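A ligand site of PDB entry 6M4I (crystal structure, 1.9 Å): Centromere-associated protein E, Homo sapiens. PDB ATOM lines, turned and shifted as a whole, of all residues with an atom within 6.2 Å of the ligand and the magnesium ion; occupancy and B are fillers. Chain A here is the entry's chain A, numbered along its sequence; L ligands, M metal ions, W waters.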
ATOM      1  N   ARG A  18      16.265   6.184  -4.585  1.00  0.00           N
ATOM      2  CA  ARG A  18      15.291   6.791  -3.687  1.00  0.00           C
ATOM      3  C   ARG A  18      15.185   8.254  -4.039  1.00  0.00           C
ATOM      4  O   ARG A  18      16.160   8.971  -3.875  1.00  0.00           O
ATOM      5  CB  ARG A  18      15.621   6.584  -2.211  1.00  0.00           C
ATOM      6  CG  ARG A  18      14.436   6.971  -1.352  1.00  0.00           C
ATOM      7  CD  ARG A  18      14.744   7.145   0.105  1.00  0.00           C
ATOM      8  NE  ARG A  18      13.492   7.318   0.811  1.00  0.00           N
ATOM      9  CZ  ARG A  18      13.334   7.307   2.116  1.00  0.00           C
ATOM     10  NH1 ARG A  18      14.357   7.109   2.956  1.00  0.00           N
ATOM     11  NH2 ARG A  18      12.116   7.468   2.590  1.00  0.00           N
ATOM     12  N   VAL A  19      14.014   8.656  -4.555  1.00  0.00           N
ATOM     13  CA  VAL A  19      13.734  10.059  -4.943  1.00  0.00           C
ATOM     14  C   VAL A  19      13.270  10.765  -3.691  1.00  0.00           C
ATOM     15  O   VAL A  19      12.332  10.277  -3.083  1.00  0.00           O
ATOM     16  CB  VAL A  19      12.673  10.155  -6.057  1.00  0.00           C
ATOM     17  CG1 VAL A  19      12.487  11.608  -6.475  1.00  0.00           C
ATOM     18  CG2 VAL A  19      13.036   9.295  -7.247  1.00  0.00           C
ATOM     19  N   ARG A  20      13.859  11.898  -3.340  1.00  0.00           N
ATOM     20  CA  ARG A  20      13.366  12.633  -2.163  1.00  0.00           C
ATOM     21  C   ARG A  20      12.188  13.517  -2.609  1.00  0.00           C
ATOM     22  O   ARG A  20      12.149  13.981  -3.750  1.00  0.00           O
ATOM     23  CB  ARG A  20      14.512  13.344  -1.452  1.00  0.00           C
ATOM     24  CG  ARG A  20      14.726  14.799  -1.802  1.00  0.00           C
ATOM     25  CD  ARG A  20      15.178  15.564  -0.560  1.00  0.00           C
ATOM     26  NE  ARG A  20      16.260  16.469  -0.932  1.00  0.00           N
ATOM     27  CZ  ARG A  20      16.117  17.570  -1.671  1.00  0.00           C
ATOM     28  NH1 ARG A  20      14.927  17.932  -2.128  1.00  0.00           N
ATOM     29  NH2 ARG A  20      17.178  18.293  -1.964  1.00  0.00           N
ATOM     30  N   PRO A  21      11.208  13.751  -1.726  1.00  0.00           N
ATOM     31  CA  PRO A  21      10.105  14.652  -2.025  1.00  0.00           C
ATOM     32  C   PRO A  21      10.635  16.095  -1.968  1.00  0.00           C
ATOM     33  O   PRO A  21      11.702  16.324  -1.426  1.00  0.00           O
ATOM     34  CB  PRO A  21       9.067  14.339  -0.939  1.00  0.00           C
ATOM     35  CG  PRO A  21       9.906  13.874   0.243  1.00  0.00           C
ATOM     36  CD  PRO A  21      11.134  13.206  -0.353  1.00  0.00           C
ATOM     37  N   ASN A  23      11.183  20.050  -1.038  1.00  0.00           N
ATOM     38  CA  ASN A  23      11.353  20.668   0.318  1.00  0.00           C
ATOM     39  C   ASN A  23      10.770  22.087   0.335  1.00  0.00           C
ATOM     40  O   ASN A  23       9.852  22.358  -0.463  1.00  0.00           O
ATOM     41  CB  ASN A  23      12.805  20.588   0.801  1.00  0.00           C
ATOM     42  CG  ASN A  23      13.738  21.630   0.195  1.00  0.00           C
ATOM     43  OD1 ASN A  23      13.309  22.539  -0.494  1.00  0.00           O
ATOM     44  ND2 ASN A  23      15.034  21.490   0.465  1.00  0.00           N
ATOM     45  N   GLY A  61       9.033   9.968  -3.881  1.00  0.00           N
ATOM     46  CA  GLY A  61       9.036  10.982  -2.796  1.00  0.00           C
ATOM     47  C   GLY A  61       8.167  10.635  -1.604  1.00  0.00           C
ATOM     48  O   GLY A  61       8.461  11.155  -0.513  1.00  0.00           O
ATOM     49  N   GLU A  63       7.447   7.422  -0.476  1.00  0.00           N
ATOM     50  CA  GLU A  63       7.737   6.088   0.150  1.00  0.00           C
ATOM     51  C   GLU A  63       8.651   6.323   1.365  1.00  0.00           C
ATOM     52  O   GLU A  63       9.448   7.275   1.337  1.00  0.00           O
ATOM     53  CB  GLU A  63       8.227   5.094  -0.896  1.00  0.00           C
ATOM     54  CG  GLU A  63       7.170   4.818  -1.950  1.00  0.00           C
ATOM     55  CD  GLU A  63       7.477   3.717  -2.948  1.00  0.00           C
ATOM     56  OE1 GLU A  63       8.103   3.979  -4.008  1.00  0.00           O
ATOM     57  OE2 GLU A  63       7.080   2.594  -2.655  1.00  0.00           O
ATOM     58  N   THR A  65      11.193   5.422   4.848  1.00  0.00           N
ATOM     59  CA  THR A  65      12.453   4.693   5.155  1.00  0.00           C
ATOM     60  C   THR A  65      12.053   3.293   5.643  1.00  0.00           C
ATOM     61  O   THR A  65      12.744   2.342   5.315  1.00  0.00           O
ATOM     62  CB  THR A  65      13.315   5.498   6.121  1.00  0.00           C
ATOM     63  OG1 THR A  65      13.232   6.829   5.618  1.00  0.00           O
ATOM     64  CG2 THR A  65      14.759   5.032   6.200  1.00  0.00           C
ATOM     65  N   GLY A  92      24.865   9.488  -3.242  1.00  0.00           N
ATOM     66  CA  GLY A  92      24.115  10.545  -3.944  1.00  0.00           C
ATOM     67  C   GLY A  92      24.605  11.894  -3.508  1.00  0.00           C
ATOM     68  O   GLY A  92      25.470  11.949  -2.624  1.00  0.00           O
ATOM     69  N   GLN A  93      24.052  12.909  -4.140  1.00  0.00           N
ATOM     70  CA  GLN A  93      24.384  14.348  -3.925  1.00  0.00           C
ATOM     71  C   GLN A  93      24.132  14.754  -2.464  1.00  0.00           C
ATOM     72  O   GLN A  93      23.189  14.225  -1.825  1.00  0.00           O
ATOM     73  CB  GLN A  93      23.493  15.126  -4.908  1.00  0.00           C
ATOM     74  CG  GLN A  93      23.688  16.619  -4.893  1.00  0.00           C
ATOM     75  CD  GLN A  93      22.651  17.375  -5.710  1.00  0.00           C
ATOM     76  OE1 GLN A  93      21.620  16.839  -6.119  1.00  0.00           O
ATOM     77  NE2 GLN A  93      22.977  18.621  -5.984  1.00  0.00           N
ATOM     78  N   THR A  94      24.868  15.724  -1.968  1.00  0.00           N
ATOM     79  CA  THR A  94      24.548  16.438  -0.691  1.00  0.00           C
ATOM     80  C   THR A  94      23.096  16.935  -0.775  1.00  0.00           C
ATOM     81  O   THR A  94      22.697  17.439  -1.856  1.00  0.00           O
ATOM     82  CB  THR A  94      25.554  17.540  -0.402  1.00  0.00           C
ATOM     83  OG1 THR A  94      26.827  16.901  -0.256  1.00  0.00           O
ATOM     84  CG2 THR A  94      25.201  18.346   0.833  1.00  0.00           C
ATOM     85  N   ALA A  95      22.343  16.729   0.301  1.00  0.00           N
ATOM     86  CA  ALA A  95      20.911  17.082   0.468  1.00  0.00           C
ATOM     87  C   ALA A  95      19.993  16.163  -0.343  1.00  0.00           C
ATOM     88  O   ALA A  95      18.781  16.524  -0.520  1.00  0.00           O
ATOM     89  CB  ALA A  95      20.701  18.543   0.123  1.00  0.00           C
ATOM     90  N   SER A  96      20.450  15.010  -0.819  1.00  0.00           N
ATOM     91  CA  SER A  96      19.582  14.093  -1.618  1.00  0.00           C
ATOM     92  C   SER A  96      18.826  13.117  -0.704  1.00  0.00           C
ATOM     93  O   SER A  96      17.830  12.554  -1.186  1.00  0.00           O
ATOM     94  CB  SER A  96      20.335  13.375  -2.685  1.00  0.00           C
ATOM     95  OG  SER A  96      21.386  12.575  -2.179  1.00  0.00           O
ATOM     96  N   GLY A  97      19.279  12.856   0.535  1.00  0.00           N
ATOM     97  CA  GLY A  97      18.590  11.890   1.403  1.00  0.00           C
ATOM     98  C   GLY A  97      19.435  10.785   2.019  1.00  0.00           C
ATOM     99  O   GLY A  97      18.808   9.869   2.597  1.00  0.00           O
ATOM    100  N   LYS A  98      20.762  10.784   1.863  1.00  0.00           N
ATOM    101  CA  LYS A  98      21.655   9.702   2.381  1.00  0.00           C
ATOM    102  C   LYS A  98      21.451   9.493   3.887  1.00  0.00           C
ATOM    103  O   LYS A  98      21.213   8.346   4.284  1.00  0.00           O
ATOM    104  CB  LYS A  98      23.120   9.971   2.071  1.00  0.00           C
ATOM    105  CG  LYS A  98      23.447   9.961   0.573  1.00  0.00           C
ATOM    106  CD  LYS A  98      24.925  10.150   0.254  1.00  0.00           C
ATOM    107  CE  LYS A  98      25.537  11.451   0.756  1.00  0.00           C
ATOM    108  NZ  LYS A  98      24.774  12.617   0.248  1.00  0.00           N
ATOM    109  N   THR A  99      21.602  10.553   4.687  1.00  0.00           N
ATOM    110  CA  THR A  99      21.572  10.517   6.163  1.00  0.00           C
ATOM    111  C   THR A  99      20.121  10.325   6.611  1.00  0.00           C
ATOM    112  O   THR A  99      19.887   9.517   7.535  1.00  0.00           O
ATOM    113  CB  THR A  99      22.262  11.753   6.774  1.00  0.00           C
ATOM    114  OG1 THR A  99      23.590  11.791   6.271  1.00  0.00           O
ATOM    115  CG2 THR A  99      22.387  11.705   8.274  1.00  0.00           C
ATOM    116  N   TYR A 100      19.165  10.946   5.891  1.00  0.00           N
ATOM    117  CA  TYR A 100      17.740  10.729   6.146  1.00  0.00           C
ATOM    118  C   TYR A 100      17.465   9.223   6.040  1.00  0.00           C
ATOM    119  O   TYR A 100      16.764   8.700   6.893  1.00  0.00           O
ATOM    120  CB  TYR A 100      16.851  11.533   5.184  1.00  0.00           C
ATOM    121  CG  TYR A 100      15.394  11.352   5.482  1.00  0.00           C
ATOM    122  CD1 TYR A 100      14.744  12.126   6.432  1.00  0.00           C
ATOM    123  CD2 TYR A 100      14.679  10.351   4.846  1.00  0.00           C
ATOM    124  CE1 TYR A 100      13.373  11.946   6.691  1.00  0.00           C
ATOM    125  CE2 TYR A 100      13.325  10.183   5.070  1.00  0.00           C
ATOM    126  CZ  TYR A 100      12.668  10.969   6.010  1.00  0.00           C
ATOM    127  OH  TYR A 100      11.350  10.717   6.246  1.00  0.00           O
ATOM    128  N   THR A 101      17.983   8.554   5.003  1.00  0.00           N
ATOM    129  CA  THR A 101      17.714   7.113   4.749  1.00  0.00           C
ATOM    130  C   THR A 101      18.478   6.219   5.758  1.00  0.00           C
ATOM    131  O   THR A 101      17.912   5.237   6.227  1.00  0.00           O
ATOM    132  CB  THR A 101      18.059   6.764   3.306  1.00  0.00           C
ATOM    133  OG1 THR A 101      17.284   7.631   2.457  1.00  0.00           O
ATOM    134  CG2 THR A 101      17.778   5.310   2.983  1.00  0.00           C
ATOM    135  N   ARG A 195      30.544  12.974  15.283  1.00  0.00           N
ATOM    136  CA  ARG A 195      30.483  13.358  13.836  1.00  0.00           C
ATOM    137  C   ARG A 195      30.082  14.840  13.777  1.00  0.00           C
ATOM    138  O   ARG A 195      30.737  15.584  13.013  1.00  0.00           O
ATOM    139  CB  ARG A 195      29.578  12.410  13.021  1.00  0.00           C
ATOM    140  CG  ARG A 195      29.207  12.913  11.626  1.00  0.00           C
ATOM    141  CD  ARG A 195      28.753  11.909  10.558  1.00  0.00           C
ATOM    142  NE  ARG A 195      27.441  11.303  10.757  1.00  0.00           N
ATOM    143  CZ  ARG A 195      26.547  10.926   9.817  1.00  0.00           C
ATOM    144  NH1 ARG A 195      26.772  11.108   8.522  1.00  0.00           N
ATOM    145  NH2 ARG A 195      25.397  10.359  10.191  1.00  0.00           N
ATOM    146  N   SER A 206      30.490  16.957   7.284  1.00  0.00           N
ATOM    147  CA  SER A 206      29.742  15.667   7.302  1.00  0.00           C
ATOM    148  C   SER A 206      29.230  15.334   5.889  1.00  0.00           C
ATOM    149  O   SER A 206      28.976  14.138   5.621  1.00  0.00           O
ATOM    150  CB  SER A 206      28.631  15.689   8.328  1.00  0.00           C
ATOM    151  OG  SER A 206      27.691  16.708   8.044  1.00  0.00           O
ATOM    152  N   SER A 207      29.124  16.341   5.018  1.00  0.00           N
ATOM    153  CA  SER A 207      28.736  16.243   3.595  1.00  0.00           C
ATOM    154  C   SER A 207      29.940  15.805   2.740  1.00  0.00           C
ATOM    155  O   SER A 207      29.730  15.425   1.597  1.00  0.00           O
ATOM    156  CB  SER A 207      28.156  17.558   3.112  1.00  0.00           C
ATOM    157  OG  SER A 207      29.198  18.419   2.659  1.00  0.00           O
ATOM    158  N   ASP A 241      27.173   5.544   4.986  1.00  0.00           N
ATOM    159  CA  ASP A 241      26.643   6.850   4.512  1.00  0.00           C
ATOM    160  C   ASP A 241      27.803   7.579   3.804  1.00  0.00           C
ATOM    161  O   ASP A 241      28.736   8.095   4.531  1.00  0.00           O
ATOM    162  CB  ASP A 241      26.028   7.586   5.712  1.00  0.00           C
ATOM    163  CG  ASP A 241      25.397   8.948   5.406  1.00  0.00           C
ATOM    164  OD1 ASP A 241      25.679   9.525   4.321  1.00  0.00           O
ATOM    165  OD2 ASP A 241      24.653   9.456   6.301  1.00  0.00           O
ATOM    166  N   LEU A 242      27.802   7.604   2.461  1.00  0.00           N
ATOM    167  CA  LEU A 242      28.953   8.172   1.692  1.00  0.00           C
ATOM    168  C   LEU A 242      28.965   9.700   1.700  1.00  0.00           C
ATOM    169  O   LEU A 242      27.954  10.356   2.096  1.00  0.00           O
ATOM    170  CB  LEU A 242      29.057   7.592   0.274  1.00  0.00           C
ATOM    171  CG  LEU A 242      29.255   6.078   0.152  1.00  0.00           C
ATOM    172  CD1 LEU A 242      28.963   5.626  -1.241  1.00  0.00           C
ATOM    173  CD2 LEU A 242      30.689   5.652   0.485  1.00  0.00           C
ATOM    174  N   THR A 313      20.432   7.969  -3.648  1.00  0.00           N
ATOM    175  CA  THR A 313      19.435   9.001  -3.279  1.00  0.00           C
ATOM    176  C   THR A 313      19.569  10.163  -4.269  1.00  0.00           C
ATOM    177  O   THR A 313      20.715  10.512  -4.650  1.00  0.00           O
ATOM    178  CB  THR A 313      19.607   9.432  -1.823  1.00  0.00           C
ATOM    179  OG1 THR A 313      20.938   9.940  -1.673  1.00  0.00           O
ATOM    180  CG2 THR A 313      19.384   8.308  -0.851  1.00  0.00           C
HETATM  181  P1  LIG L   1      22.450  14.096   2.616  1.00  0.00           P
HETATM  182  O1  LIG L   1      22.385  13.198   1.436  1.00  0.00           O
HETATM  183  O2  LIG L   1      22.755  13.329   3.922  1.00  0.00           O
HETATM  184  O3  LIG L   1      23.310  15.270   2.426  1.00  0.00           O
HETATM  185  P2  LIG L   1      19.988  14.515   4.155  1.00  0.00           P
HETATM  186  O4  LIG L   1      19.654  13.092   4.387  1.00  0.00           O
HETATM  187  O5  LIG L   1      20.557  15.325   5.247  1.00  0.00           O
HETATM  188  O6  LIG L   1      20.933  14.608   2.855  1.00  0.00           O
HETATM  189  O7  LIG L   1      18.629  15.205   3.588  1.00  0.00           O
HETATM  190  C1  LIG L   1      18.532  16.621   3.329  1.00  0.00           C
HETATM  191  C2  LIG L   1      17.254  17.167   3.930  1.00  0.00           C
HETATM  192  O8  LIG L   1      16.099  16.615   3.246  1.00  0.00           O
HETATM  193  C3  LIG L   1      17.034  16.847   5.413  1.00  0.00           C
HETATM  194  O9  LIG L   1      16.361  17.917   6.058  1.00  0.00           O
HETATM  195  C4  LIG L   1      16.180  15.580   5.352  1.00  0.00           C
HETATM  196  O10 LIG L   1      15.368  15.332   6.478  1.00  0.00           O
HETATM  197  C5  LIG L   1      15.315  15.861   4.141  1.00  0.00           C
HETATM  198  N1  LIG L   1      14.904  14.618   3.477  1.00  0.00           N
HETATM  199  C6  LIG L   1      15.725  13.808   2.749  1.00  0.00           C
HETATM  200  N2  LIG L   1      15.132  12.753   2.271  1.00  0.00           N
HETATM  201  C7  LIG L   1      13.817  12.889   2.689  1.00  0.00           C
HETATM  202  C8  LIG L   1      12.693  12.092   2.459  1.00  0.00           C
HETATM  203  N3  LIG L   1      12.738  10.962   1.755  1.00  0.00           N
HETATM  204  N4  LIG L   1      11.520  12.495   3.015  1.00  0.00           N
HETATM  205  C9  LIG L   1      11.524  13.626   3.733  1.00  0.00           C
HETATM  206  N5  LIG L   1      12.508  14.476   3.982  1.00  0.00           N
HETATM  207  C10 LIG L   1      13.658  14.039   3.426  1.00  0.00           C
HETATM  208 MG    MG M   1      24.292  13.492   5.148  1.00  0.00          MG
HETATM  209  O   HOH W   1      25.684  11.960   4.451  1.00  0.00           O
HETATM  210  O   HOH W   2      19.311  14.408   7.608  1.00  0.00           O
HETATM  211  O   HOH W   3      25.256  15.047   3.976  1.00  0.00           O
HETATM  212  O   HOH W   4      26.522  14.474   1.310  1.00  0.00           O
HETATM  213  O   HOH W   5      25.711  13.740   6.650  1.00  0.00           O
HETATM  214  O   HOH W   6      15.382  10.085   1.172  1.00  0.00           O
HETATM  215  O   HOH W   7      22.836  14.778   6.056  1.00  0.00           O
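O4 of the ligand sits at hydrogen-bond distance from N of Thr 99 (3.2 Å). The backbone NH (N) of Tyr 100 sits at hydrogen-bond distance from an oxygen (O4) of the ligand (2.7 Å). The backbone NH (N) of Lys 98 sits at hydrogen-bond distance from an oxygen (O1) of the ligand (2.9 Å). The side-chain amino group (NZ) of Lys 98 is in salt-bridge range of an oxygen (O1) of the ligand. N of Ala 95 sits at hydrogen-bond distance from O3 of the ligand, 2.8 Å away. The backbone NH (N) of Gly 97 is in hydrogen-bond range of an oxygen (O1) of the ligand. An oxygen (O1) of the ligand lies within hydrogen-bond range of the backbone NH (N) of Ser 96, 3.5 Å away.
The side-chain carboxylate of Asp 241 lies close to the side-chain hydroxyl of Thr 99 (2.6 Å). NZ of Lys 98 is in hydrogen-bond range of O of Gly 92 (3.0 Å). The guanidinium group (NE) of Arg 20 sits at hydrogen-bond distance from the backbone carbonyl oxygen (O) of Ala 95 (2.6 Å). OG1 of Thr 101 sits at hydrogen-bond distance from O of Gly 97 (2.7 Å). OG of Ser 96 sits at hydrogen-bond distance from O of Gln 93 (2.5 Å). The side-chain hydroxyl (OG) of Ser 96 sits at hydrogen-bond distance from the side-chain hydroxyl (OG1) of Thr 313. NH1 of Arg 18 sits at hydrogen-bond distance from OG1 of Thr 101 (3.0 Å). OG1 of Thr 65 sits at hydrogen-bond distance from NH1 of Arg 18 (2.9 Å).
Residues that only touch the ligand: Arg 18, Arg 20, Pro 21, Gln 93 and Thr 94. Hydrophobic or aromatic side chains that line the ligand: Pro 21 and Tyr 100. Of the 24 residues printed, 11 come within 4 Å of the ligand. The nearest printed residue that does not touch the ligand is Thr 313 (4.7 Å).
The nearest printed residue that does not touch the magnesium ion is Asp 241 (4.2 Å).
The magnesium ion is bound by an oxygen (O2) of the ligand, 2.0 Å away. Water W5 binds the magnesium ion, 2.1 Å away. Water W7 binds the magnesium ion, 2.1 Å away. OG1 of Thr 99 is bound to the magnesium ion (2.2 Å). Water W3 binds the magnesium ion (2.2 Å). Water W1 binds the magnesium ion (2.2 Å). The magnesium ion has six donor atoms within binding distance.
Water W5 lies within hydrogen-bond range of the guanidinium group of Arg 195 and the backbone carbonyl oxygen of Ser 206. Water W6 lies within hydrogen-bond range of a nitrogen (N3) of the ligand, the side-chain hydroxyl (OG1) of Thr 101 and the guanidinium group (NE) of Arg 18. Water W4 lies within hydrogen-bond range of NZ of Lys 98 (2.8 Å), OG1 of Thr 94 (2.9 Å), O of Ser 207 (3.4 Å) and O3 of the ligand (3.5 Å).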
